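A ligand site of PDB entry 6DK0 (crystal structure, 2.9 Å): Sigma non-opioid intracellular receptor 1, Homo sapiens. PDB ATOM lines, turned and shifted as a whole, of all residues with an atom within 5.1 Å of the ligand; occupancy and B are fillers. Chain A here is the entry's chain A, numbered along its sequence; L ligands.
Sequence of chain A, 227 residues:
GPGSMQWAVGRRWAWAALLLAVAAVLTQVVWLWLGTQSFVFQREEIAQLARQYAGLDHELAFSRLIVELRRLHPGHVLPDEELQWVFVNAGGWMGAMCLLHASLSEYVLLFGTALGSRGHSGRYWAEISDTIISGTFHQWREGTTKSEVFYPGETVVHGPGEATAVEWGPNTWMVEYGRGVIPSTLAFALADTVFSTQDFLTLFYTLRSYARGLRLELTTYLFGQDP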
ATOM      1  N   VAL A  88     -17.563   3.242  10.917  1.00  0.00           N
ATOM      2  CA  VAL A  88     -17.860   3.773  12.247  1.00  0.00           C
ATOM      3  C   VAL A  88     -19.339   4.082  12.288  1.00  0.00           C
ATOM      4  O   VAL A  88     -19.805   4.991  11.584  1.00  0.00           O
ATOM      5  CB  VAL A  88     -17.036   5.021  12.581  1.00  0.00           C
ATOM      6  CG1 VAL A  88     -17.569   5.682  13.837  1.00  0.00           C
ATOM      7  CG2 VAL A  88     -15.572   4.655  12.758  1.00  0.00           C
ATOM      8  N   TRP A  93     -25.472   7.804  12.929  1.00  0.00           N
ATOM      9  CA  TRP A  93     -24.814   8.030  11.652  1.00  0.00           C
ATOM     10  C   TRP A  93     -23.757   6.961  11.393  1.00  0.00           C
ATOM     11  O   TRP A  93     -23.345   6.225  12.285  1.00  0.00           O
ATOM     12  CB  TRP A  93     -24.180   9.426  11.593  1.00  0.00           C
ATOM     13  CG  TRP A  93     -23.290   9.765  12.751  1.00  0.00           C
ATOM     14  CD1 TRP A  93     -23.615  10.536  13.831  1.00  0.00           C
ATOM     15  CD2 TRP A  93     -21.922   9.359  12.937  1.00  0.00           C
ATOM     16  NE1 TRP A  93     -22.534  10.632  14.685  1.00  0.00           N
ATOM     17  CE2 TRP A  93     -21.490   9.922  14.161  1.00  0.00           C
ATOM     18  CE3 TRP A  93     -21.028   8.575  12.195  1.00  0.00           C
ATOM     19  CZ2 TRP A  93     -20.207   9.714  14.654  1.00  0.00           C
ATOM     20  CZ3 TRP A  93     -19.756   8.379  12.692  1.00  0.00           C
ATOM     21  CH2 TRP A  93     -19.355   8.947  13.909  1.00  0.00           C
ATOM     22  N   MET A  97     -13.394   5.916   8.937  1.00  0.00           N
ATOM     23  CA  MET A  97     -12.213   6.633   9.396  1.00  0.00           C
ATOM     24  C   MET A  97     -10.958   5.807   9.172  1.00  0.00           C
ATOM     25  O   MET A  97     -10.992   4.570   9.134  1.00  0.00           O
ATOM     26  CB  MET A  97     -12.307   7.018  10.882  1.00  0.00           C
ATOM     27  CG  MET A  97     -12.428   5.855  11.847  1.00  0.00           C
ATOM     28  SD  MET A  97     -10.865   5.126  12.392  1.00  0.00           S
ATOM     29  CE  MET A  97     -10.147   6.471  13.320  1.00  0.00           C
ATOM     30  N   LEU A  99      -7.094   5.961  10.898  1.00  0.00           N
ATOM     31  CA  LEU A  99      -6.355   6.549  12.000  1.00  0.00           C
ATOM     32  C   LEU A  99      -4.895   6.750  11.616  1.00  0.00           C
ATOM     33  O   LEU A  99      -4.220   5.790  11.231  1.00  0.00           O
ATOM     34  CB  LEU A  99      -6.476   5.654  13.235  1.00  0.00           C
ATOM     35  CG  LEU A  99      -5.760   6.111  14.503  1.00  0.00           C
ATOM     36  CD1 LEU A  99      -6.376   7.392  15.036  1.00  0.00           C
ATOM     37  CD2 LEU A  99      -5.822   5.007  15.547  1.00  0.00           C
ATOM     38  N   ALA A 102      -2.651   8.350  17.328  1.00  0.00           N
ATOM     39  CA  ALA A 102      -3.566   8.214  18.459  1.00  0.00           C
ATOM     40  C   ALA A 102      -2.769   7.932  19.709  1.00  0.00           C
ATOM     41  O   ALA A 102      -2.053   6.932  19.779  1.00  0.00           O
ATOM     42  CB  ALA A 102      -4.585   7.103  18.211  1.00  0.00           C
ATOM     43  N   TYR A 107      -5.429  12.581  18.896  1.00  0.00           N
ATOM     44  CA  TYR A 107      -5.620  11.686  17.770  1.00  0.00           C
ATOM     45  C   TYR A 107      -5.760  12.510  16.494  1.00  0.00           C
ATOM     46  O   TYR A 107      -6.275  13.633  16.511  1.00  0.00           O
ATOM     47  CB  TYR A 107      -6.840  10.764  17.943  1.00  0.00           C
ATOM     48  CG  TYR A 107      -8.213  11.410  17.825  1.00  0.00           C
ATOM     49  CD1 TYR A 107      -8.760  11.711  16.586  1.00  0.00           C
ATOM     50  CD2 TYR A 107      -8.969  11.682  18.948  1.00  0.00           C
ATOM     51  CE1 TYR A 107     -10.004  12.292  16.472  1.00  0.00           C
ATOM     52  CE2 TYR A 107     -10.223  12.258  18.847  1.00  0.00           C
ATOM     53  CZ  TYR A 107     -10.729  12.560  17.601  1.00  0.00           C
ATOM     54  OH  TYR A 107     -11.982  13.131  17.491  1.00  0.00           O
ATOM     55  N   LEU A 109      -7.088  11.689  12.408  1.00  0.00           N
ATOM     56  CA  LEU A 109      -7.694  10.694  11.542  1.00  0.00           C
ATOM     57  C   LEU A 109      -8.260  11.368  10.302  1.00  0.00           C
ATOM     58  O   LEU A 109      -8.379  12.587  10.228  1.00  0.00           O
ATOM     59  CB  LEU A 109      -8.769   9.884  12.286  1.00  0.00           C
ATOM     60  CG  LEU A 109      -9.962  10.607  12.909  1.00  0.00           C
ATOM     61  CD1 LEU A 109     -11.091  10.786  11.897  1.00  0.00           C
ATOM     62  CD2 LEU A 109     -10.474   9.853  14.124  1.00  0.00           C
ATOM     63  N   PHE A 111     -11.765  11.195   8.166  1.00  0.00           N
ATOM     64  CA  PHE A 111     -13.141  10.749   8.347  1.00  0.00           C
ATOM     65  C   PHE A 111     -13.966  11.154   7.144  1.00  0.00           C
ATOM     66  O   PHE A 111     -13.636  12.087   6.414  1.00  0.00           O
ATOM     67  CB  PHE A 111     -13.745  11.329   9.637  1.00  0.00           C
ATOM     68  CG  PHE A 111     -15.119  10.823   9.940  1.00  0.00           C
ATOM     69  CD1 PHE A 111     -15.307   9.576  10.498  1.00  0.00           C
ATOM     70  CD2 PHE A 111     -16.228  11.599   9.652  1.00  0.00           C
ATOM     71  CE1 PHE A 111     -16.572   9.101  10.775  1.00  0.00           C
ATOM     72  CE2 PHE A 111     -17.495  11.138   9.934  1.00  0.00           C
ATOM     73  CZ  PHE A 111     -17.673   9.893  10.493  1.00  0.00           C
ATOM     74  N   SER A 121     -23.759  14.117  17.201  1.00  0.00           N
ATOM     75  CA  SER A 121     -22.325  14.379  17.133  1.00  0.00           C
ATOM     76  C   SER A 121     -21.572  13.651  18.233  1.00  0.00           C
ATOM     77  O   SER A 121     -20.389  13.336  18.067  1.00  0.00           O
ATOM     78  CB  SER A 121     -22.047  15.879  17.236  1.00  0.00           C
ATOM     79  OG  SER A 121     -22.265  16.353  18.549  1.00  0.00           O
ATOM     80  N   TYR A 124     -18.551  14.387  24.043  1.00  0.00           N
ATOM     81  CA  TYR A 124     -17.209  13.903  24.345  1.00  0.00           C
ATOM     82  C   TYR A 124     -16.588  14.653  25.519  1.00  0.00           C
ATOM     83  O   TYR A 124     -17.027  15.730  25.908  1.00  0.00           O
ATOM     84  CB  TYR A 124     -16.291  14.047  23.120  1.00  0.00           C
ATOM     85  CG  TYR A 124     -16.854  13.506  21.834  1.00  0.00           C
ATOM     86  CD1 TYR A 124     -17.097  12.149  21.674  1.00  0.00           C
ATOM     87  CD2 TYR A 124     -17.119  14.349  20.770  1.00  0.00           C
ATOM     88  CE1 TYR A 124     -17.601  11.649  20.499  1.00  0.00           C
ATOM     89  CE2 TYR A 124     -17.614  13.864  19.578  1.00  0.00           C
ATOM     90  CZ  TYR A 124     -17.860  12.512  19.449  1.00  0.00           C
ATOM     91  OH  TYR A 124     -18.353  12.018  18.261  1.00  0.00           O
ATOM     92  N   ILE A 128     -12.703  18.649  19.482  1.00  0.00           N
ATOM     93  CA  ILE A 128     -12.533  18.007  18.181  1.00  0.00           C
ATOM     94  C   ILE A 128     -12.515  19.077  17.104  1.00  0.00           C
ATOM     95  O   ILE A 128     -13.294  20.035  17.161  1.00  0.00           O
ATOM     96  CB  ILE A 128     -13.644  16.979  17.913  1.00  0.00           C
ATOM     97  CG1 ILE A 128     -13.915  16.145  19.166  1.00  0.00           C
ATOM     98  CG2 ILE A 128     -13.256  16.071  16.776  1.00  0.00           C
ATOM     99  CD1 ILE A 128     -12.731  15.323  19.655  1.00  0.00           C
ATOM    100  N   ASP A 130     -12.471  19.545  12.846  1.00  0.00           N
ATOM    101  CA  ASP A 130     -12.675  18.894  11.560  1.00  0.00           C
ATOM    102  C   ASP A 130     -12.487  19.918  10.449  1.00  0.00           C
ATOM    103  O   ASP A 130     -13.240  20.895  10.363  1.00  0.00           O
ATOM    104  CB  ASP A 130     -14.074  18.282  11.473  1.00  0.00           C
ATOM    105  CG  ASP A 130     -14.154  16.935  12.164  1.00  0.00           C
ATOM    106  OD1 ASP A 130     -13.580  15.968  11.634  1.00  0.00           O
ATOM    107  OD2 ASP A 130     -14.779  16.854  13.235  1.00  0.00           O
ATOM    108  N   PHE A 137     -20.746  20.023   5.555  1.00  0.00           N
ATOM    109  CA  PHE A 137     -20.961  19.619   6.945  1.00  0.00           C
ATOM    110  C   PHE A 137     -21.991  20.554   7.570  1.00  0.00           C
ATOM    111  O   PHE A 137     -21.697  21.734   7.793  1.00  0.00           O
ATOM    112  CB  PHE A 137     -19.645  19.646   7.728  1.00  0.00           C
ATOM    113  CG  PHE A 137     -19.804  19.318   9.188  1.00  0.00           C
ATOM    114  CD1 PHE A 137     -19.874  18.004   9.614  1.00  0.00           C
ATOM    115  CD2 PHE A 137     -19.881  20.327  10.131  1.00  0.00           C
ATOM    116  CE1 PHE A 137     -20.019  17.702  10.949  1.00  0.00           C
ATOM    117  CE2 PHE A 137     -20.028  20.030  11.474  1.00  0.00           C
ATOM    118  CZ  PHE A 137     -20.095  18.707  11.883  1.00  0.00           C
ATOM    119  N   HIS A 158     -15.801  21.300  17.760  1.00  0.00           N
ATOM    120  CA  HIS A 158     -16.778  20.741  18.682  1.00  0.00           C
ATOM    121  C   HIS A 158     -16.124  20.714  20.055  1.00  0.00           C
ATOM    122  O   HIS A 158     -15.222  19.909  20.308  1.00  0.00           O
ATOM    123  CB  HIS A 158     -17.202  19.341  18.238  1.00  0.00           C
ATOM    124  CG  HIS A 158     -18.404  18.815  18.945  1.00  0.00           C
ATOM    125  ND1 HIS A 158     -19.656  19.386  18.813  1.00  0.00           N
ATOM    126  CD2 HIS A 158     -18.561  17.758  19.772  1.00  0.00           C
ATOM    127  CE1 HIS A 158     -20.524  18.702  19.541  1.00  0.00           C
ATOM    128  NE2 HIS A 158     -19.890  17.719  20.135  1.00  0.00           N
ATOM    129  N   VAL A 166     -25.532  16.473  13.445  1.00  0.00           N
ATOM    130  CA  VAL A 166     -24.602  16.563  12.328  1.00  0.00           C
ATOM    131  C   VAL A 166     -25.216  15.930  11.095  1.00  0.00           C
ATOM    132  O   VAL A 166     -25.980  14.955  11.182  1.00  0.00           O
ATOM    133  CB  VAL A 166     -23.250  15.905  12.664  1.00  0.00           C
ATOM    134  CG1 VAL A 166     -22.530  16.729  13.722  1.00  0.00           C
ATOM    135  CG2 VAL A 166     -23.449  14.480  13.143  1.00  0.00           C
ATOM    136  N   TRP A 168     -23.717  15.077   7.118  1.00  0.00           N
ATOM    137  CA  TRP A 168     -22.749  15.095   6.031  1.00  0.00           C
ATOM    138  C   TRP A 168     -23.464  14.800   4.726  1.00  0.00           C
ATOM    139  O   TRP A 168     -24.159  13.771   4.612  1.00  0.00           O
ATOM    140  CB  TRP A 168     -21.626  14.085   6.259  1.00  0.00           C
ATOM    141  CG  TRP A 168     -20.968  14.197   7.595  1.00  0.00           C
ATOM    142  CD1 TRP A 168     -20.099  15.160   8.002  1.00  0.00           C
ATOM    143  CD2 TRP A 168     -21.100  13.289   8.699  1.00  0.00           C
ATOM    144  NE1 TRP A 168     -19.694  14.921   9.282  1.00  0.00           N
ATOM    145  CE2 TRP A 168     -20.294  13.780   9.735  1.00  0.00           C
ATOM    146  CE3 TRP A 168     -21.833  12.116   8.903  1.00  0.00           C
ATOM    147  CZ2 TRP A 168     -20.198  13.148  10.975  1.00  0.00           C
ATOM    148  CZ3 TRP A 168     -21.737  11.489  10.129  1.00  0.00           C
ATOM    149  CH2 TRP A 168     -20.922  11.995  11.147  1.00  0.00           C
ATOM    150  N   MET A 174     -13.058  14.736   5.446  1.00  0.00           N
ATOM    151  CA  MET A 174     -12.433  15.747   6.295  1.00  0.00           C
ATOM    152  C   MET A 174     -11.291  15.119   7.076  1.00  0.00           C
ATOM    153  O   MET A 174     -11.173  13.896   7.185  1.00  0.00           O
ATOM    154  CB  MET A 174     -13.457  16.346   7.274  1.00  0.00           C
ATOM    155  CG  MET A 174     -13.972  15.326   8.263  1.00  0.00           C
ATOM    156  SD  MET A 174     -15.585  15.769   8.932  1.00  0.00           S
ATOM    157  CE  MET A 174     -16.596  15.634   7.473  1.00  0.00           C
ATOM    158  N   GLU A 176      -9.622  15.104  10.863  1.00  0.00           N
ATOM    159  CA  GLU A 176     -10.053  15.343  12.225  1.00  0.00           C
ATOM    160  C   GLU A 176      -8.864  15.271  13.167  1.00  0.00           C
ATOM    161  O   GLU A 176      -8.029  14.360  13.082  1.00  0.00           O
ATOM    162  CB  GLU A 176     -11.104  14.327  12.659  1.00  0.00           C
ATOM    163  CG  GLU A 176     -11.778  14.663  13.974  1.00  0.00           C
ATOM    164  CD  GLU A 176     -13.003  13.815  14.244  1.00  0.00           C
ATOM    165  OE1 GLU A 176     -12.954  12.981  15.175  1.00  0.00           O
ATOM    166  OE2 GLU A 176     -14.017  13.983  13.535  1.00  0.00           O
ATOM    167  N   ILE A 182      -9.127  10.668  25.258  1.00  0.00           N
ATOM    168  CA  ILE A 182      -9.482   9.899  24.059  1.00  0.00           C
ATOM    169  C   ILE A 182     -10.205   8.600  24.385  1.00  0.00           C
ATOM    170  O   ILE A 182     -11.171   8.264  23.679  1.00  0.00           O
ATOM    171  CB  ILE A 182      -8.241   9.683  23.183  1.00  0.00           C
ATOM    172  CG1 ILE A 182      -7.519  11.016  22.963  1.00  0.00           C
ATOM    173  CG2 ILE A 182      -8.618   9.057  21.851  1.00  0.00           C
ATOM    174  CD1 ILE A 182      -8.400  12.110  22.372  1.00  0.00           C
ATOM    175  N   THR A 185     -14.199   8.675  24.244  1.00  0.00           N
ATOM    176  CA  THR A 185     -14.943   8.715  23.000  1.00  0.00           C
ATOM    177  C   THR A 185     -15.229   7.317  22.448  1.00  0.00           C
ATOM    178  O   THR A 185     -16.133   7.164  21.622  1.00  0.00           O
ATOM    179  CB  THR A 185     -14.183   9.523  21.946  1.00  0.00           C
ATOM    180  OG1 THR A 185     -13.014   8.809  21.542  1.00  0.00           O
ATOM    181  CG2 THR A 185     -13.780  10.873  22.515  1.00  0.00           C
ATOM    182  N   LEU A 186     -14.472   6.303  22.892  1.00  0.00           N
ATOM    183  CA  LEU A 186     -14.687   4.956  22.379  1.00  0.00           C
ATOM    184  C   LEU A 186     -16.070   4.422  22.740  1.00  0.00           C
ATOM    185  O   LEU A 186     -16.637   3.615  21.986  1.00  0.00           O
ATOM    186  CB  LEU A 186     -13.589   4.015  22.896  1.00  0.00           C
ATOM    187  N   ALA A 189     -18.352   6.011  20.172  1.00  0.00           N
ATOM    188  CA  ALA A 189     -18.015   5.647  18.807  1.00  0.00           C
ATOM    189  C   ALA A 189     -18.369   4.209  18.471  1.00  0.00           C
ATOM    190  O   ALA A 189     -18.520   3.869  17.292  1.00  0.00           O
ATOM    191  CB  ALA A 189     -16.518   5.896  18.550  1.00  0.00           C
ATOM    192  N   THR A 206     -11.392  -1.528  14.818  1.00  0.00           N
ATOM    193  CA  THR A 206     -11.228  -0.248  15.494  1.00  0.00           C
ATOM    194  C   THR A 206     -10.288  -0.371  16.692  1.00  0.00           C
ATOM    195  O   THR A 206      -9.355   0.437  16.858  1.00  0.00           O
ATOM    196  CB  THR A 206     -12.587   0.283  15.935  1.00  0.00           C
ATOM    197  OG1 THR A 206     -13.502   0.263  14.825  1.00  0.00           O
ATOM    198  CG2 THR A 206     -12.464   1.708  16.464  1.00  0.00           C
ATOM    199  N   TYR A 210      -6.534   1.393  17.252  1.00  0.00           N
ATOM    200  CA  TYR A 210      -6.166   2.141  18.452  1.00  0.00           C
ATOM    201  C   TYR A 210      -4.920   1.539  19.108  1.00  0.00           C
ATOM    202  O   TYR A 210      -4.010   2.267  19.516  1.00  0.00           O
ATOM    203  CB  TYR A 210      -7.336   2.162  19.437  1.00  0.00           C
ATOM    204  CG  TYR A 210      -7.215   3.231  20.499  1.00  0.00           C
ATOM    205  CD1 TYR A 210      -6.573   4.430  20.236  1.00  0.00           C
ATOM    206  CD2 TYR A 210      -7.745   3.035  21.765  1.00  0.00           C
ATOM    207  CE1 TYR A 210      -6.457   5.416  21.204  1.00  0.00           C
ATOM    208  CE2 TYR A 210      -7.637   4.002  22.742  1.00  0.00           C
ATOM    209  CZ  TYR A 210      -6.992   5.192  22.461  1.00  0.00           C
ATOM    210  OH  TYR A 210      -6.884   6.163  23.425  1.00  0.00           O
HETATM  211  C1  LIG L   1     -15.369  10.776  15.042  1.00  0.00           C
HETATM  212  C2  LIG L   1     -10.675   7.390  18.718  1.00  0.00           C
HETATM  213  C3  LIG L   1     -15.516   9.632  14.275  1.00  0.00           C
HETATM  214  C4  LIG L   1     -16.487  17.140  15.611  1.00  0.00           C
HETATM  215  C5  LIG L   1     -17.062  16.171  16.646  1.00  0.00           C
HETATM  216  C6  LIG L   1     -17.797  14.979  16.034  1.00  0.00           C
HETATM  217  C7  LIG L   1     -17.698  14.018  13.860  1.00  0.00           C
HETATM  218  C8  LIG L   1     -18.203  15.329  13.239  1.00  0.00           C
HETATM  219  C9  LIG L   1     -17.405  15.709  11.990  1.00  0.00           C
HETATM  220  C10 LIG L   1     -16.407  13.059  15.665  1.00  0.00           C
HETATM  221  C11 LIG L   1     -16.020  12.065  14.560  1.00  0.00           C
HETATM  222  C12 LIG L   1     -14.640  10.723  16.222  1.00  0.00           C
HETATM  223  C13 LIG L   1     -14.048   9.532  16.623  1.00  0.00           C
HETATM  224  C14 LIG L   1     -11.924   9.333  17.612  1.00  0.00           C
HETATM  225  C15 LIG L   1     -11.286   8.783  18.900  1.00  0.00           C
HETATM  226  C16 LIG L   1      -9.428   7.237  18.115  1.00  0.00           C
HETATM  227  C17 LIG L   1      -8.876   5.977  17.959  1.00  0.00           C
HETATM  228  C18 LIG L   1      -9.570   4.860  18.410  1.00  0.00           C
HETATM  229  C19 LIG L   1     -10.806   5.009  19.005  1.00  0.00           C
HETATM  230  C20 LIG L   1     -11.358   6.269  19.161  1.00  0.00           C
HETATM  231  C21 LIG L   1     -14.204   8.383  15.847  1.00  0.00           C
HETATM  232  C22 LIG L   1     -14.268   6.018  15.807  1.00  0.00           C
HETATM  233  C23 LIG L   1     -14.933   8.435  14.667  1.00  0.00           C
HETATM  234  N1  LIG L   1     -16.943  14.285  15.083  1.00  0.00           N
HETATM  235  O1  LIG L   1     -13.309   9.477  17.818  1.00  0.00           O
HETATM  236  O2  LIG L   1     -13.620   7.177  16.243  1.00  0.00           O
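CG2 of Val 88 touches C22 of the ligand, 3.6 Å away. Trp 93 touches the ligand (CH2 to C3, 3.9 Å). Tyr 107 touches the ligand (CZ to C14, 3.4 Å). Leu 109 touches the ligand. Phe 111 touches the ligand. O of Ser 121 touches C6 of the ligand, 3.7 Å away. OH of Tyr 124 touches C10 of the ligand (3.4 Å). Ile 128 touches the ligand. Phe 137 touches the ligand. His 158 touches the ligand (CB to C4, 3.5 Å). Trp 168 touches the ligand (NE1 to C9, 3.6 Å). Met 174 touches the ligand. CG2 of Ile 182 touches C15 of the ligand, at 3.99 Å. Thr 185 touches the ligand (OG1 to C15, 3.2 Å). Ala 189 touches the ligand (CB to C22, 3.5 Å). CD1 of Tyr 210 touches C18 of the ligand, 3.5 Å away. Hydrophobic or aromatic side chains within 4 Å of the ligand: Val 88, Trp 93, Tyr 107, Leu 109, Phe 111, Tyr 124, Ile 128, Phe 137, His 158, Trp 168, Met 174, Ile 182, Ala 189 and Tyr 210. Within 4 Å of the ligand: Val 88, Trp 93, Tyr 107, Leu 109, Phe 111, Ser 121, Tyr 124, Ile 128, Asp 130, Phe 137, His 158, Trp 168, Met 174, Glu 176, Ile 182, Thr 185, Ala 189 and Tyr 210. The nearest printed residue that does not touch the ligand is Leu 99 (4.01 Å).
The side-chain hydroxyl (OG) of Ser 121 lies close to a ring nitrogen (NE2) of His 158. The backbone NH (N) of Glu 176 lies within hydrogen-bond range of the backbone carbonyl oxygen (O) of Leu 109. OE1 of Glu 176 lies within hydrogen-bond range of OH of Tyr 107 (2.5 Å). The side-chain hydroxyl (OH) of Tyr 124 lies within hydrogen-bond range of the backbone carbonyl oxygen (O) of Ser 121 (2.4 Å). The backbone NH (N) of Met 174 sits at hydrogen-bond distance from the backbone carbonyl oxygen (O) of Phe 111 (2.9 Å). O of Ile 128 sits at hydrogen-bond distance from N of His 158. OG1 of Thr 185 lies within hydrogen-bond range of O of Ile 182, 2.9 Å away.
The side-chain carboxylate of Glu 176 is in salt-bridge range of a nitrogen (N1) of the ligand (3.3 Å). A nitrogen (N1) of the ligand is in salt-bridge range of the side-chain carboxylate (OD2) of Asp 130 (3.8 Å).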
